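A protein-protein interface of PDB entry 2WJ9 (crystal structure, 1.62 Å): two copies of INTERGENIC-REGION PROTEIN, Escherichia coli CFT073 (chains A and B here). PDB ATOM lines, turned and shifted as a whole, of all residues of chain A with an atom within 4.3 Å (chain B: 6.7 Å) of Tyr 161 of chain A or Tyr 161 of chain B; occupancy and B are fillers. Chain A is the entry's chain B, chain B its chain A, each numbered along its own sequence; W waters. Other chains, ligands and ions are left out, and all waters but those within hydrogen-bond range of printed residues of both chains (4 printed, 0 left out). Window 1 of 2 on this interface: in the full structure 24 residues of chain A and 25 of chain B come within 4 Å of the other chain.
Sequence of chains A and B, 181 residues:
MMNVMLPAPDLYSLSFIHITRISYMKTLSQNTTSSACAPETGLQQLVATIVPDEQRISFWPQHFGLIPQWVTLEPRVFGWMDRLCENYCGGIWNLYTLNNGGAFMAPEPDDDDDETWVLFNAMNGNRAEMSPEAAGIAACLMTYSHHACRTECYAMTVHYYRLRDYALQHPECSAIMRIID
Hydrophobic or aromatic side chains of chain B that line the printed part of chain A: Ala 36, Ala 38, Val 158 and Tyr 161.
Of the 9 printed residues of chain A, 7 touch a printed residue of chain B.
Printed residues of chain A that touch a printed residue of chain B: Thr 157, Val 158, Tyr 160, Tyr 161, Arg 162, Arg 164 and Asp 165.
Among the printed residues, 15 pairs touch across the chains.
Water W2 lies within hydrogen-bond range of OH of Tyr 161 of chain B and NE of Arg 162 of chain A.
Water W1 lies within hydrogen-bond range of OD2 of Asp 165 of chain A (2.7 Å) and OH of Tyr 161 of chain B (2.9 Å).
Water W3 lies within hydrogen-bond range of OE2 of Glu 40 of chain B (2.8 Å), O of Asn 100 of chain B (2.8 Å), NH2 of Arg 162 of chain B (3.1 Å) and OH of Tyr 161 of chain A (3.4 Å).
Water W4 lies within hydrogen-bond range of O of Ala 38 of chain B (2.8 Å), OH of Tyr 160 of chain A (3.2 Å) and O of Pro 39 of chain B (3.3 Å).
CB of Thr 157 of chain A touches CG2 of Val 158 of chain B, 3.9 Å away.
Val 158 of chain A touches Thr 157 of chain B (CG2 to CB, 3.7 Å).
Val 158 of chain A touches Val 158 of chain B.
Tyr 160 of chain A touches Ala 38 of chain B (CE2 to O, 3.9 Å).
Tyr 161 of chain A touches Ala 38 of chain B.
CG of Tyr 161 of chain B touches CB of Tyr 161 of chain A (3.9 Å).
OH of Tyr 161 of chain B touches CG of Arg 162 of chain A (3.4 Å).
Arg 164 of chain A touches Glu 40 of chain B.
Asp 165 of chain A touches Tyr 161 of chain B.
Thr 157 of chain A touches Val 158 of chain B, and with the chains exchanged Val 158 of chain A touches Thr 157 of chain B.
Val 158 of chain A touches its own counterpart, Val 158 of chain B.
Tyr 161 of chain A touches its own counterpart, Tyr 161 of chain B.
Asp 165 of chain A touches Tyr 161 of chain B, but with the chains exchanged Tyr 161 of chain A does not touch Asp 165 of chain B (4.4 Å).
Positions printed for both chains: 157, 158, 159, 160, 161, 162, 163, 164 and 165.
O of Arg 162 of chain B lies within hydrogen-bond range of ND2 of Asn 100 of chain B.
The side-chain carboxylate of Asp 165 of chain B lies within salt-bridge range of the guanidinium group of Arg 164 of chain B.
O of Cys 37 of chain B sits at hydrogen-bond distance from NH2 of Arg 162 of chain B, 3.5 Å away.
OE1 of Glu 40 of chain B is in hydrogen-bond range of OH of Tyr 161 of chain A (2.7 Å).
The guanidinium group (NH1) of Arg 164 of chain B lies within salt-bridge range of the side-chain carboxylate (OD2) of Asp 165 of chain A, 2.8 Å away.
The guanidinium group (NE) of Arg 162 of chain B lies within hydrogen-bond range of the side-chain hydroxyl (OH) of Tyr 161 of chain A, at 3.1 Å.
The backbone carbonyl oxygen (O) of Ala 36 of chain B lies within hydrogen-bond range of the side-chain hydroxyl (OG1) of Thr 157 of chain A (2.6 Å).
OD2 of Asp 165 of chain B is in salt-bridge range of NH1 of Arg 164 of chain A, at 2.9 Å.
The backbone carbonyl oxygen of Glu 40 of chain B is in hydrogen-bond range of the side-chain hydroxyl of Tyr 160 of chain A (2.8 Å).
Tyr 161 of chain A touches just these residues of chain B: Ala 38, Glu 40, Tyr 161 and Arg 162.
Tyr 161 of chain B touches just these residues of chain A: Tyr 161 (3.9 Å), Arg 162 (3.4 Å) and Asp 165 (3.5 Å).
Of the printed residues of chain A, Asp 165 of chain B touches Arg 164 (2.9 Å).
Of the printed residues of chain B, Thr 157 of chain A touches Ala 36 and Val 158.
Of the printed residues of chain B, Val 158 of chain A touches Thr 157 (3.7 Å) and Val 158 (3.8 Å).
Of the printed residues of chain A, Glu 40 of chain B touches Tyr 160 (2.8 Å), Tyr 161 (2.7 Å) and Arg 164 (3.9 Å).
His 159 of chain B touches none of the printed residues of chain A.
Tyr 144 of chain B touches none of the printed residues of chain A.
The nearest residue of chain B that does not touch Tyr 161 of chain A is Val 158 of chain B (4.1 Å).
The nearest printed residue of chain A that does not touch Tyr 161 of chain B is Val 158 of chain A (5.0 Å).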
ATOM      1  N   THR A 157      -5.713  11.787   8.904  1.00  0.00           N
ATOM      2  CA  THR A 157      -4.549  12.218   8.104  1.00  0.00           C
ATOM      3  C   THR A 157      -3.309  11.358   8.393  1.00  0.00           C
ATOM      4  O   THR A 157      -2.596  10.927   7.477  1.00  0.00           O
ATOM      5  CB  THR A 157      -4.192  13.717   8.351  1.00  0.00           C
ATOM      6  OG1 THR A 157      -5.380  14.512   8.490  1.00  0.00           O
ATOM      7  CG2 THR A 157      -3.327  14.284   7.216  1.00  0.00           C
ATOM      8  N   VAL A 158      -3.039  11.103   9.673  1.00  0.00           N
ATOM      9  CA  VAL A 158      -1.900  10.270  10.027  1.00  0.00           C
ATOM     10  C   VAL A 158      -2.017   8.827   9.499  1.00  0.00           C
ATOM     11  O   VAL A 158      -1.041   8.293   8.975  1.00  0.00           O
ATOM     12  CB  VAL A 158      -1.641  10.304  11.540  1.00  0.00           C
ATOM     13  CG1 VAL A 158      -0.642   9.221  11.947  1.00  0.00           C
ATOM     14  CG2 VAL A 158      -1.172  11.707  11.959  1.00  0.00           C
ATOM     15  N   HIS A 159      -3.199   8.222   9.604  1.00  0.00           N
ATOM     16  CA  HIS A 159      -3.457   6.921   8.964  1.00  0.00           C
ATOM     17  C   HIS A 159      -3.161   6.957   7.450  1.00  0.00           C
ATOM     18  O   HIS A 159      -2.560   6.025   6.904  1.00  0.00           O
ATOM     19  CB  HIS A 159      -4.890   6.430   9.235  1.00  0.00           C
ATOM     20  CG  HIS A 159      -5.020   5.601  10.479  1.00  0.00           C
ATOM     21  ND1 HIS A 159      -4.343   4.412  10.654  1.00  0.00           N
ATOM     22  CD2 HIS A 159      -5.746   5.789  11.608  1.00  0.00           C
ATOM     23  CE1 HIS A 159      -4.631   3.912  11.844  1.00  0.00           C
ATOM     24  NE2 HIS A 159      -5.487   4.724  12.442  1.00  0.00           N
ATOM     25  N   TYR A 160      -3.564   8.035   6.776  1.00  0.00           N
ATOM     26  CA  TYR A 160      -3.256   8.191   5.356  1.00  0.00           C
ATOM     27  C   TYR A 160      -1.748   8.218   5.078  1.00  0.00           C
ATOM     28  O   TYR A 160      -1.259   7.474   4.224  1.00  0.00           O
ATOM     29  CB  TYR A 160      -3.909   9.453   4.785  1.00  0.00           C
ATOM     30  CG  TYR A 160      -3.576   9.681   3.318  1.00  0.00           C
ATOM     31  CD1 TYR A 160      -4.070   8.824   2.346  1.00  0.00           C
ATOM     32  CD2 TYR A 160      -2.745  10.720   2.914  1.00  0.00           C
ATOM     33  CE1 TYR A 160      -3.763   8.997   1.004  1.00  0.00           C
ATOM     34  CE2 TYR A 160      -2.435  10.916   1.556  1.00  0.00           C
ATOM     35  CZ  TYR A 160      -2.949  10.041   0.606  1.00  0.00           C
ATOM     36  OH  TYR A 160      -2.657  10.213  -0.747  1.00  0.00           O
ATOM     37  N   TYR A 161      -1.010   9.062   5.802  1.00  0.00           N
ATOM     38  CA  TYR A 161       0.447   9.163   5.600  1.00  0.00           C
ATOM     39  C   TYR A 161       1.153   7.820   5.907  1.00  0.00           C
ATOM     40  O   TYR A 161       2.078   7.415   5.211  1.00  0.00           O
ATOM     41  CB  TYR A 161       1.057  10.315   6.431  1.00  0.00           C
ATOM     42  CG  TYR A 161       0.890  11.703   5.823  1.00  0.00           C
ATOM     43  CD1 TYR A 161       0.124  12.672   6.453  1.00  0.00           C
ATOM     44  CD2 TYR A 161       1.524  12.056   4.627  1.00  0.00           C
ATOM     45  CE1 TYR A 161      -0.036  13.943   5.904  1.00  0.00           C
ATOM     46  CE2 TYR A 161       1.368  13.332   4.076  1.00  0.00           C
ATOM     47  CZ  TYR A 161       0.581  14.261   4.717  1.00  0.00           C
ATOM     48  OH  TYR A 161       0.410  15.524   4.194  1.00  0.00           O
ATOM     49  N   ARG A 162       0.691   7.118   6.931  1.00  0.00           N
ATOM     50  CA  ARG A 162       1.331   5.859   7.338  1.00  0.00           C
ATOM     51  C   ARG A 162       1.136   4.740   6.303  1.00  0.00           C
ATOM     52  O   ARG A 162       2.083   4.031   5.957  1.00  0.00           O
ATOM     53  CB  ARG A 162       0.859   5.445   8.732  1.00  0.00           C
ATOM     54  CG  ARG A 162       1.509   6.306   9.816  1.00  0.00           C
ATOM     55  CD  ARG A 162       0.935   6.074  11.191  1.00  0.00           C
ATOM     56  NE  ARG A 162       1.720   6.784  12.200  1.00  0.00           N
ATOM     57  CZ  ARG A 162       1.391   6.898  13.481  1.00  0.00           C
ATOM     58  NH1 ARG A 162       0.266   6.362  13.943  1.00  0.00           N
ATOM     59  NH2 ARG A 162       2.202   7.557  14.301  1.00  0.00           N
ATOM     60  N   LEU A 163      -0.082   4.602   5.800  1.00  0.00           N
ATOM     61  CA  LEU A 163      -0.357   3.645   4.713  1.00  0.00           C
ATOM     62  C   LEU A 163       0.299   4.058   3.386  1.00  0.00           C
ATOM     63  O   LEU A 163       0.784   3.198   2.636  1.00  0.00           O
ATOM     64  CB  LEU A 163      -1.865   3.442   4.534  1.00  0.00           C
ATOM     65  CG  LEU A 163      -2.309   2.380   3.515  1.00  0.00           C
ATOM     66  CD1 LEU A 163      -1.802   0.987   3.901  1.00  0.00           C
ATOM     67  CD2 LEU A 163      -3.840   2.404   3.366  1.00  0.00           C
ATOM     68  N   ARG A 164       0.302   5.359   3.088  1.00  0.00           N
ATOM     69  CA  ARG A 164       0.989   5.884   1.909  1.00  0.00           C
ATOM     70  C   ARG A 164       2.462   5.464   1.892  1.00  0.00           C
ATOM     71  O   ARG A 164       2.975   5.071   0.857  1.00  0.00           O
ATOM     72  CB  ARG A 164       0.843   7.417   1.818  1.00  0.00           C
ATOM     73  CG  ARG A 164       1.603   8.115   0.677  1.00  0.00           C
ATOM     74  CD  ARG A 164       1.272   9.619   0.715  1.00  0.00           C
ATOM     75  NE  ARG A 164       2.039  10.475  -0.193  1.00  0.00           N
ATOM     76  CZ  ARG A 164       3.054  11.273   0.146  1.00  0.00           C
ATOM     77  NH1 ARG A 164       3.506  11.331   1.396  1.00  0.00           N
ATOM     78  NH2 ARG A 164       3.631  12.023  -0.783  1.00  0.00           N
ATOM     79  N   ASP A 165       3.137   5.528   3.044  1.00  0.00           N
ATOM     80  CA  ASP A 165       4.544   5.088   3.118  1.00  0.00           C
ATOM     81  C   ASP A 165       4.718   3.600   2.782  1.00  0.00           C
ATOM     82  O   ASP A 165       5.654   3.230   2.078  1.00  0.00           O
ATOM     83  CB  ASP A 165       5.143   5.355   4.506  1.00  0.00           C
ATOM     84  CG  ASP A 165       5.633   6.779   4.685  1.00  0.00           C
ATOM     85  OD1 ASP A 165       5.493   7.617   3.761  1.00  0.00           O
ATOM     86  OD2 ASP A 165       6.189   7.058   5.775  1.00  0.00           O
ATOM     87  N   ALA B  36      -6.051  19.374   7.947  1.00  0.00           N
ATOM     88  CA  ALA B  36      -5.921  17.920   8.000  1.00  0.00           C
ATOM     89  C   ALA B  36      -6.152  17.256   6.627  1.00  0.00           C
ATOM     90  O   ALA B  36      -5.895  16.066   6.467  1.00  0.00           O
ATOM     91  CB  ALA B  36      -6.891  17.353   9.027  1.00  0.00           C
ATOM     92  N   CYS B  37      -6.645  18.015   5.645  1.00  0.00           N
ATOM     93  CA  CYS B  37      -6.820  17.504   4.292  1.00  0.00           C
ATOM     94  C   CYS B  37      -5.470  17.442   3.563  1.00  0.00           C
ATOM     95  O   CYS B  37      -4.811  18.475   3.366  1.00  0.00           O
ATOM     96  CB  CYS B  37      -7.804  18.397   3.519  1.00  0.00           C
ATOM     97  SG  CYS B  37      -8.258  17.862   1.845  1.00  0.00           S
ATOM     98  N   ALA B  38      -5.071  16.231   3.173  1.00  0.00           N
ATOM     99  CA  ALA B  38      -3.797  15.986   2.479  1.00  0.00           C
ATOM    100  C   ALA B  38      -4.059  15.473   1.066  1.00  0.00           C
ATOM    101  O   ALA B  38      -4.318  14.280   0.890  1.00  0.00           O
ATOM    102  CB  ALA B  38      -2.959  14.962   3.259  1.00  0.00           C
ATOM    103  N   PRO B  39      -4.002  16.368   0.054  1.00  0.00           N
ATOM    104  CA  PRO B  39      -4.325  16.006  -1.329  1.00  0.00           C
ATOM    105  C   PRO B  39      -3.230  15.271  -2.121  1.00  0.00           C
ATOM    106  O   PRO B  39      -3.522  14.709  -3.184  1.00  0.00           O
ATOM    107  CB  PRO B  39      -4.606  17.364  -1.977  1.00  0.00           C
ATOM    108  CG  PRO B  39      -3.743  18.309  -1.249  1.00  0.00           C
ATOM    109  CD  PRO B  39      -3.647  17.797   0.170  1.00  0.00           C
ATOM    110  N   GLU B  40      -1.995  15.270  -1.625  1.00  0.00           N
ATOM    111  CA  GLU B  40      -0.895  14.669  -2.373  1.00  0.00           C
ATOM    112  C   GLU B  40      -0.966  13.137  -2.336  1.00  0.00           C
ATOM    113  O   GLU B  40      -1.301  12.547  -1.308  1.00  0.00           O
ATOM    114  CB  GLU B  40       0.469  15.186  -1.891  1.00  0.00           C
ATOM    115  CG  GLU B  40       0.904  14.747  -0.489  1.00  0.00           C
ATOM    116  CD  GLU B  40       0.465  15.688   0.620  1.00  0.00           C
ATOM    117  OE1 GLU B  40       1.167  15.723   1.653  1.00  0.00           O
ATOM    118  OE2 GLU B  40      -0.576  16.366   0.484  1.00  0.00           O
ATOM    119  N   ASN B 100       2.916  21.817   0.763  1.00  0.00           N
ATOM    120  CA  ASN B 100       2.081  20.710   1.263  1.00  0.00           C
ATOM    121  C   ASN B 100       1.435  21.020   2.622  1.00  0.00           C
ATOM    122  O   ASN B 100       0.832  20.145   3.244  1.00  0.00           O
ATOM    123  CB  ASN B 100       2.877  19.391   1.335  1.00  0.00           C
ATOM    124  CG  ASN B 100       4.036  19.432   2.332  1.00  0.00           C
ATOM    125  OD1 ASN B 100       4.310  20.461   2.943  1.00  0.00           O
ATOM    126  ND2 ASN B 100       4.734  18.309   2.469  1.00  0.00           N
ATOM    127  N   LEU B 141      12.533  18.535  12.655  1.00  0.00           N
ATOM    128  CA  LEU B 141      11.985  17.165  12.602  1.00  0.00           C
ATOM    129  C   LEU B 141      12.031  16.466  13.971  1.00  0.00           C
ATOM    130  O   LEU B 141      11.068  15.798  14.360  1.00  0.00           O
ATOM    131  CB  LEU B 141      12.699  16.311  11.549  1.00  0.00           C
ATOM    132  CG  LEU B 141      12.361  16.623  10.088  1.00  0.00           C
ATOM    133  CD1 LEU B 141      13.365  15.961   9.166  1.00  0.00           C
ATOM    134  CD2 LEU B 141      10.920  16.227   9.728  1.00  0.00           C
ATOM    135  N   TYR B 144       9.384  18.237  16.288  1.00  0.00           N
ATOM    136  CA  TYR B 144       8.000  17.874  15.956  1.00  0.00           C
ATOM    137  C   TYR B 144       7.666  16.440  16.380  1.00  0.00           C
ATOM    138  O   TYR B 144       6.622  16.181  16.978  1.00  0.00           O
ATOM    139  CB  TYR B 144       7.714  18.036  14.454  1.00  0.00           C
ATOM    140  CG  TYR B 144       7.871  19.432  13.844  1.00  0.00           C
ATOM    141  CD1 TYR B 144       8.034  20.580  14.622  1.00  0.00           C
ATOM    142  CD2 TYR B 144       7.816  19.594  12.465  1.00  0.00           C
ATOM    143  CE1 TYR B 144       8.168  21.851  14.029  1.00  0.00           C
ATOM    144  CE2 TYR B 144       7.935  20.850  11.867  1.00  0.00           C
ATOM    145  CZ  TYR B 144       8.119  21.974  12.650  1.00  0.00           C
ATOM    146  OH  TYR B 144       8.254  23.216  12.064  1.00  0.00           O
ATOM    147  N   MET B 156       0.708  17.462  15.172  1.00  0.00           N
ATOM    148  CA  MET B 156       2.165  17.514  15.267  1.00  0.00           C
ATOM    149  C   MET B 156       2.817  16.403  14.423  1.00  0.00           C
ATOM    150  O   MET B 156       3.842  16.631  13.785  1.00  0.00           O
ATOM    151  CB  MET B 156       2.611  17.435  16.733  1.00  0.00           C
ATOM    152  CG  MET B 156       4.060  17.841  16.982  1.00  0.00           C
ATOM    153  SD  MET B 156       4.383  19.618  17.119  1.00  0.00           S
ATOM    154  CE  MET B 156       4.568  20.065  15.398  1.00  0.00           C
ATOM    155  N   THR B 157       2.221  15.209  14.430  1.00  0.00           N
ATOM    156  CA  THR B 157       2.650  14.092  13.570  1.00  0.00           C
ATOM    157  C   THR B 157       2.556  14.470  12.083  1.00  0.00           C
ATOM    158  O   THR B 157       3.436  14.147  11.288  1.00  0.00           O
ATOM    159  CB  THR B 157       1.775  12.841  13.813  1.00  0.00           C
ATOM    160  OG1 THR B 157       1.614  12.623  15.222  1.00  0.00           O
ATOM    161  CG2 THR B 157       2.375  11.587  13.154  1.00  0.00           C
ATOM    162  N   VAL B 158       1.479  15.160  11.719  1.00  0.00           N
ATOM    163  CA  VAL B 158       1.300  15.628  10.341  1.00  0.00           C
ATOM    164  C   VAL B 158       2.401  16.643   9.953  1.00  0.00           C
ATOM    165  O   VAL B 158       2.952  16.580   8.851  1.00  0.00           O
ATOM    166  CB  VAL B 158      -0.112  16.225  10.146  1.00  0.00           C
ATOM    167  CG1 VAL B 158      -0.266  16.897   8.761  1.00  0.00           C
ATOM    168  CG2 VAL B 158      -1.168  15.138  10.338  1.00  0.00           C
ATOM    169  N   HIS B 159       2.718  17.577  10.851  1.00  0.00           N
ATOM    170  CA  HIS B 159       3.868  18.487  10.643  1.00  0.00           C
ATOM    171  C   HIS B 159       5.185  17.715  10.428  1.00  0.00           C
ATOM    172  O   HIS B 159       5.980  18.061   9.538  1.00  0.00           O
ATOM    173  CB  HIS B 159       4.008  19.499  11.797  1.00  0.00           C
ATOM    174  CG  HIS B 159       3.247  20.771  11.593  1.00  0.00           C
ATOM    175  ND1 HIS B 159       3.532  21.648  10.570  1.00  0.00           N
ATOM    176  CD2 HIS B 159       2.229  21.330  12.294  1.00  0.00           C
ATOM    177  CE1 HIS B 159       2.711  22.684  10.636  1.00  0.00           C
ATOM    178  NE2 HIS B 159       1.911  22.515  11.675  1.00  0.00           N
ATOM    179  N   TYR B 160       5.415  16.663  11.219  1.00  0.00           N
ATOM    180  CA  TYR B 160       6.569  15.786  10.980  1.00  0.00           C
ATOM    181  C   TYR B 160       6.594  15.216   9.571  1.00  0.00           C
ATOM    182  O   TYR B 160       7.605  15.336   8.879  1.00  0.00           O
ATOM    183  CB  TYR B 160       6.656  14.628  11.980  1.00  0.00           C
ATOM    184  CG  TYR B 160       7.675  13.586  11.541  1.00  0.00           C
ATOM    185  CD1 TYR B 160       9.035  13.740  11.822  1.00  0.00           C
ATOM    186  CD2 TYR B 160       7.286  12.474  10.790  1.00  0.00           C
ATOM    187  CE1 TYR B 160       9.973  12.802  11.391  1.00  0.00           C
ATOM    188  CE2 TYR B 160       8.215  11.538  10.348  1.00  0.00           C
ATOM    189  CZ  TYR B 160       9.556  11.698  10.656  1.00  0.00           C
ATOM    190  OH  TYR B 160      10.467  10.761  10.209  1.00  0.00           O
ATOM    191  N   TYR B 161       5.506  14.575   9.146  1.00  0.00           N
ATOM    192  CA  TYR B 161       5.446  13.989   7.788  1.00  0.00           C
ATOM    193  C   TYR B 161       5.640  14.992   6.651  1.00  0.00           C
ATOM    194  O   TYR B 161       6.354  14.708   5.689  1.00  0.00           O
ATOM    195  CB  TYR B 161       4.141  13.199   7.582  1.00  0.00           C
ATOM    196  CG  TYR B 161       4.226  11.797   8.142  1.00  0.00           C
ATOM    197  CD1 TYR B 161       3.688  11.478   9.384  1.00  0.00           C
ATOM    198  CD2 TYR B 161       4.860  10.787   7.418  1.00  0.00           C
ATOM    199  CE1 TYR B 161       3.779  10.173   9.897  1.00  0.00           C
ATOM    200  CE2 TYR B 161       4.952   9.488   7.912  1.00  0.00           C
ATOM    201  CZ  TYR B 161       4.421   9.194   9.154  1.00  0.00           C
ATOM    202  OH  TYR B 161       4.531   7.908   9.642  1.00  0.00           O
ATOM    203  N   ARG B 162       5.016  16.156   6.777  1.00  0.00           N
ATOM    204  CA  ARG B 162       5.054  17.185   5.736  1.00  0.00           C
ATOM    205  C   ARG B 162       6.451  17.774   5.550  1.00  0.00           C
ATOM    206  O   ARG B 162       6.889  17.991   4.413  1.00  0.00           O
ATOM    207  CB  ARG B 162       4.019  18.271   6.036  1.00  0.00           C
ATOM    208  CG  ARG B 162       2.621  17.804   5.670  1.00  0.00           C
ATOM    209  CD  ARG B 162       1.526  18.668   6.212  1.00  0.00           C
ATOM    210  NE  ARG B 162       0.227  18.232   5.698  1.00  0.00           N
ATOM    211  CZ  ARG B 162      -0.951  18.761   6.035  1.00  0.00           C
ATOM    212  NH1 ARG B 162      -1.023  19.763   6.908  1.00  0.00           N
ATOM    213  NH2 ARG B 162      -2.065  18.284   5.469  1.00  0.00           N
ATOM    214  N   LEU B 163       7.153  18.003   6.663  1.00  0.00           N
ATOM    215  CA  LEU B 163       8.547  18.453   6.612  1.00  0.00           C
ATOM    216  C   LEU B 163       9.466  17.323   6.174  1.00  0.00           C
ATOM    217  O   LEU B 163      10.419  17.534   5.429  1.00  0.00           O
ATOM    218  CB  LEU B 163       9.005  18.990   7.974  1.00  0.00           C
ATOM    219  CG  LEU B 163      10.457  19.481   8.065  1.00  0.00           C
ATOM    220  CD1 LEU B 163      10.769  20.550   7.019  1.00  0.00           C
ATOM    221  CD2 LEU B 163      10.756  19.989   9.480  1.00  0.00           C
ATOM    222  N   ARG B 164       9.185  16.116   6.646  1.00  0.00           N
ATOM    223  CA  ARG B 164       9.978  14.954   6.261  1.00  0.00           C
ATOM    224  C   ARG B 164       9.967  14.735   4.746  1.00  0.00           C
ATOM    225  O   ARG B 164      11.009  14.434   4.149  1.00  0.00           O
ATOM    226  CB  ARG B 164       9.485  13.704   6.974  1.00  0.00           C
ATOM    227  CG  ARG B 164      10.414  12.516   6.808  1.00  0.00           C
ATOM    228  CD  ARG B 164       9.679  11.234   6.731  1.00  0.00           C
ATOM    229  NE  ARG B 164       8.741  11.177   5.602  1.00  0.00           N
ATOM    230  CZ  ARG B 164       7.974  10.131   5.345  1.00  0.00           C
ATOM    231  NH1 ARG B 164       8.051   9.059   6.114  1.00  0.00           N
ATOM    232  NH2 ARG B 164       7.124  10.150   4.326  1.00  0.00           N
ATOM    233  N   ASP B 165       8.805  14.910   4.117  1.00  0.00           N
ATOM    234  CA  ASP B 165       8.705  14.778   2.663  1.00  0.00           C
ATOM    235  C   ASP B 165       9.560  15.812   1.922  1.00  0.00           C
ATOM    236  O   ASP B 165      10.143  15.505   0.882  1.00  0.00           O
ATOM    237  CB  ASP B 165       7.250  14.881   2.194  1.00  0.00           C
ATOM    238  CG  ASP B 165       6.465  13.589   2.378  1.00  0.00           C
ATOM    239  OD1 ASP B 165       7.022  12.563   2.828  1.00  0.00           O
ATOM    240  OD2 ASP B 165       5.264  13.609   2.042  1.00  0.00           O
ATOM    241  N   TYR B 166       9.639  17.030   2.453  1.00  0.00           N
ATOM    242  CA  TYR B 166      10.570  18.033   1.924  1.00  0.00           C
ATOM    243  C   TYR B 166      12.021  17.557   2.059  1.00  0.00           C
ATOM    244  O   TYR B 166      12.798  17.667   1.116  1.00  0.00           O
ATOM    245  CB  TYR B 166      10.377  19.396   2.604  1.00  0.00           C
ATOM    246  CG  TYR B 166      11.289  20.496   2.073  1.00  0.00           C
ATOM    247  CD1 TYR B 166      11.179  20.963   0.763  1.00  0.00           C
ATOM    248  CD2 TYR B 166      12.249  21.088   2.896  1.00  0.00           C
ATOM    249  CE1 TYR B 166      12.015  21.981   0.283  1.00  0.00           C
ATOM    250  CE2 TYR B 166      13.085  22.105   2.426  1.00  0.00           C
ATOM    251  CZ  TYR B 166      12.965  22.543   1.124  1.00  0.00           C
ATOM    252  OH  TYR B 166      13.799  23.543   0.673  1.00  0.00           O
HETATM  253  O   HOH W   1       5.941   5.835   8.167  1.00  0.00           O
HETATM  254  O   HOH W   2       4.659   7.967  12.048  1.00  0.00           O
HETATM  255  O   HOH W   3      -1.030  18.173   2.535  1.00  0.00           O
HETATM  256  O   HOH W   4      -4.905  12.461  -1.193  1.00  0.00           O
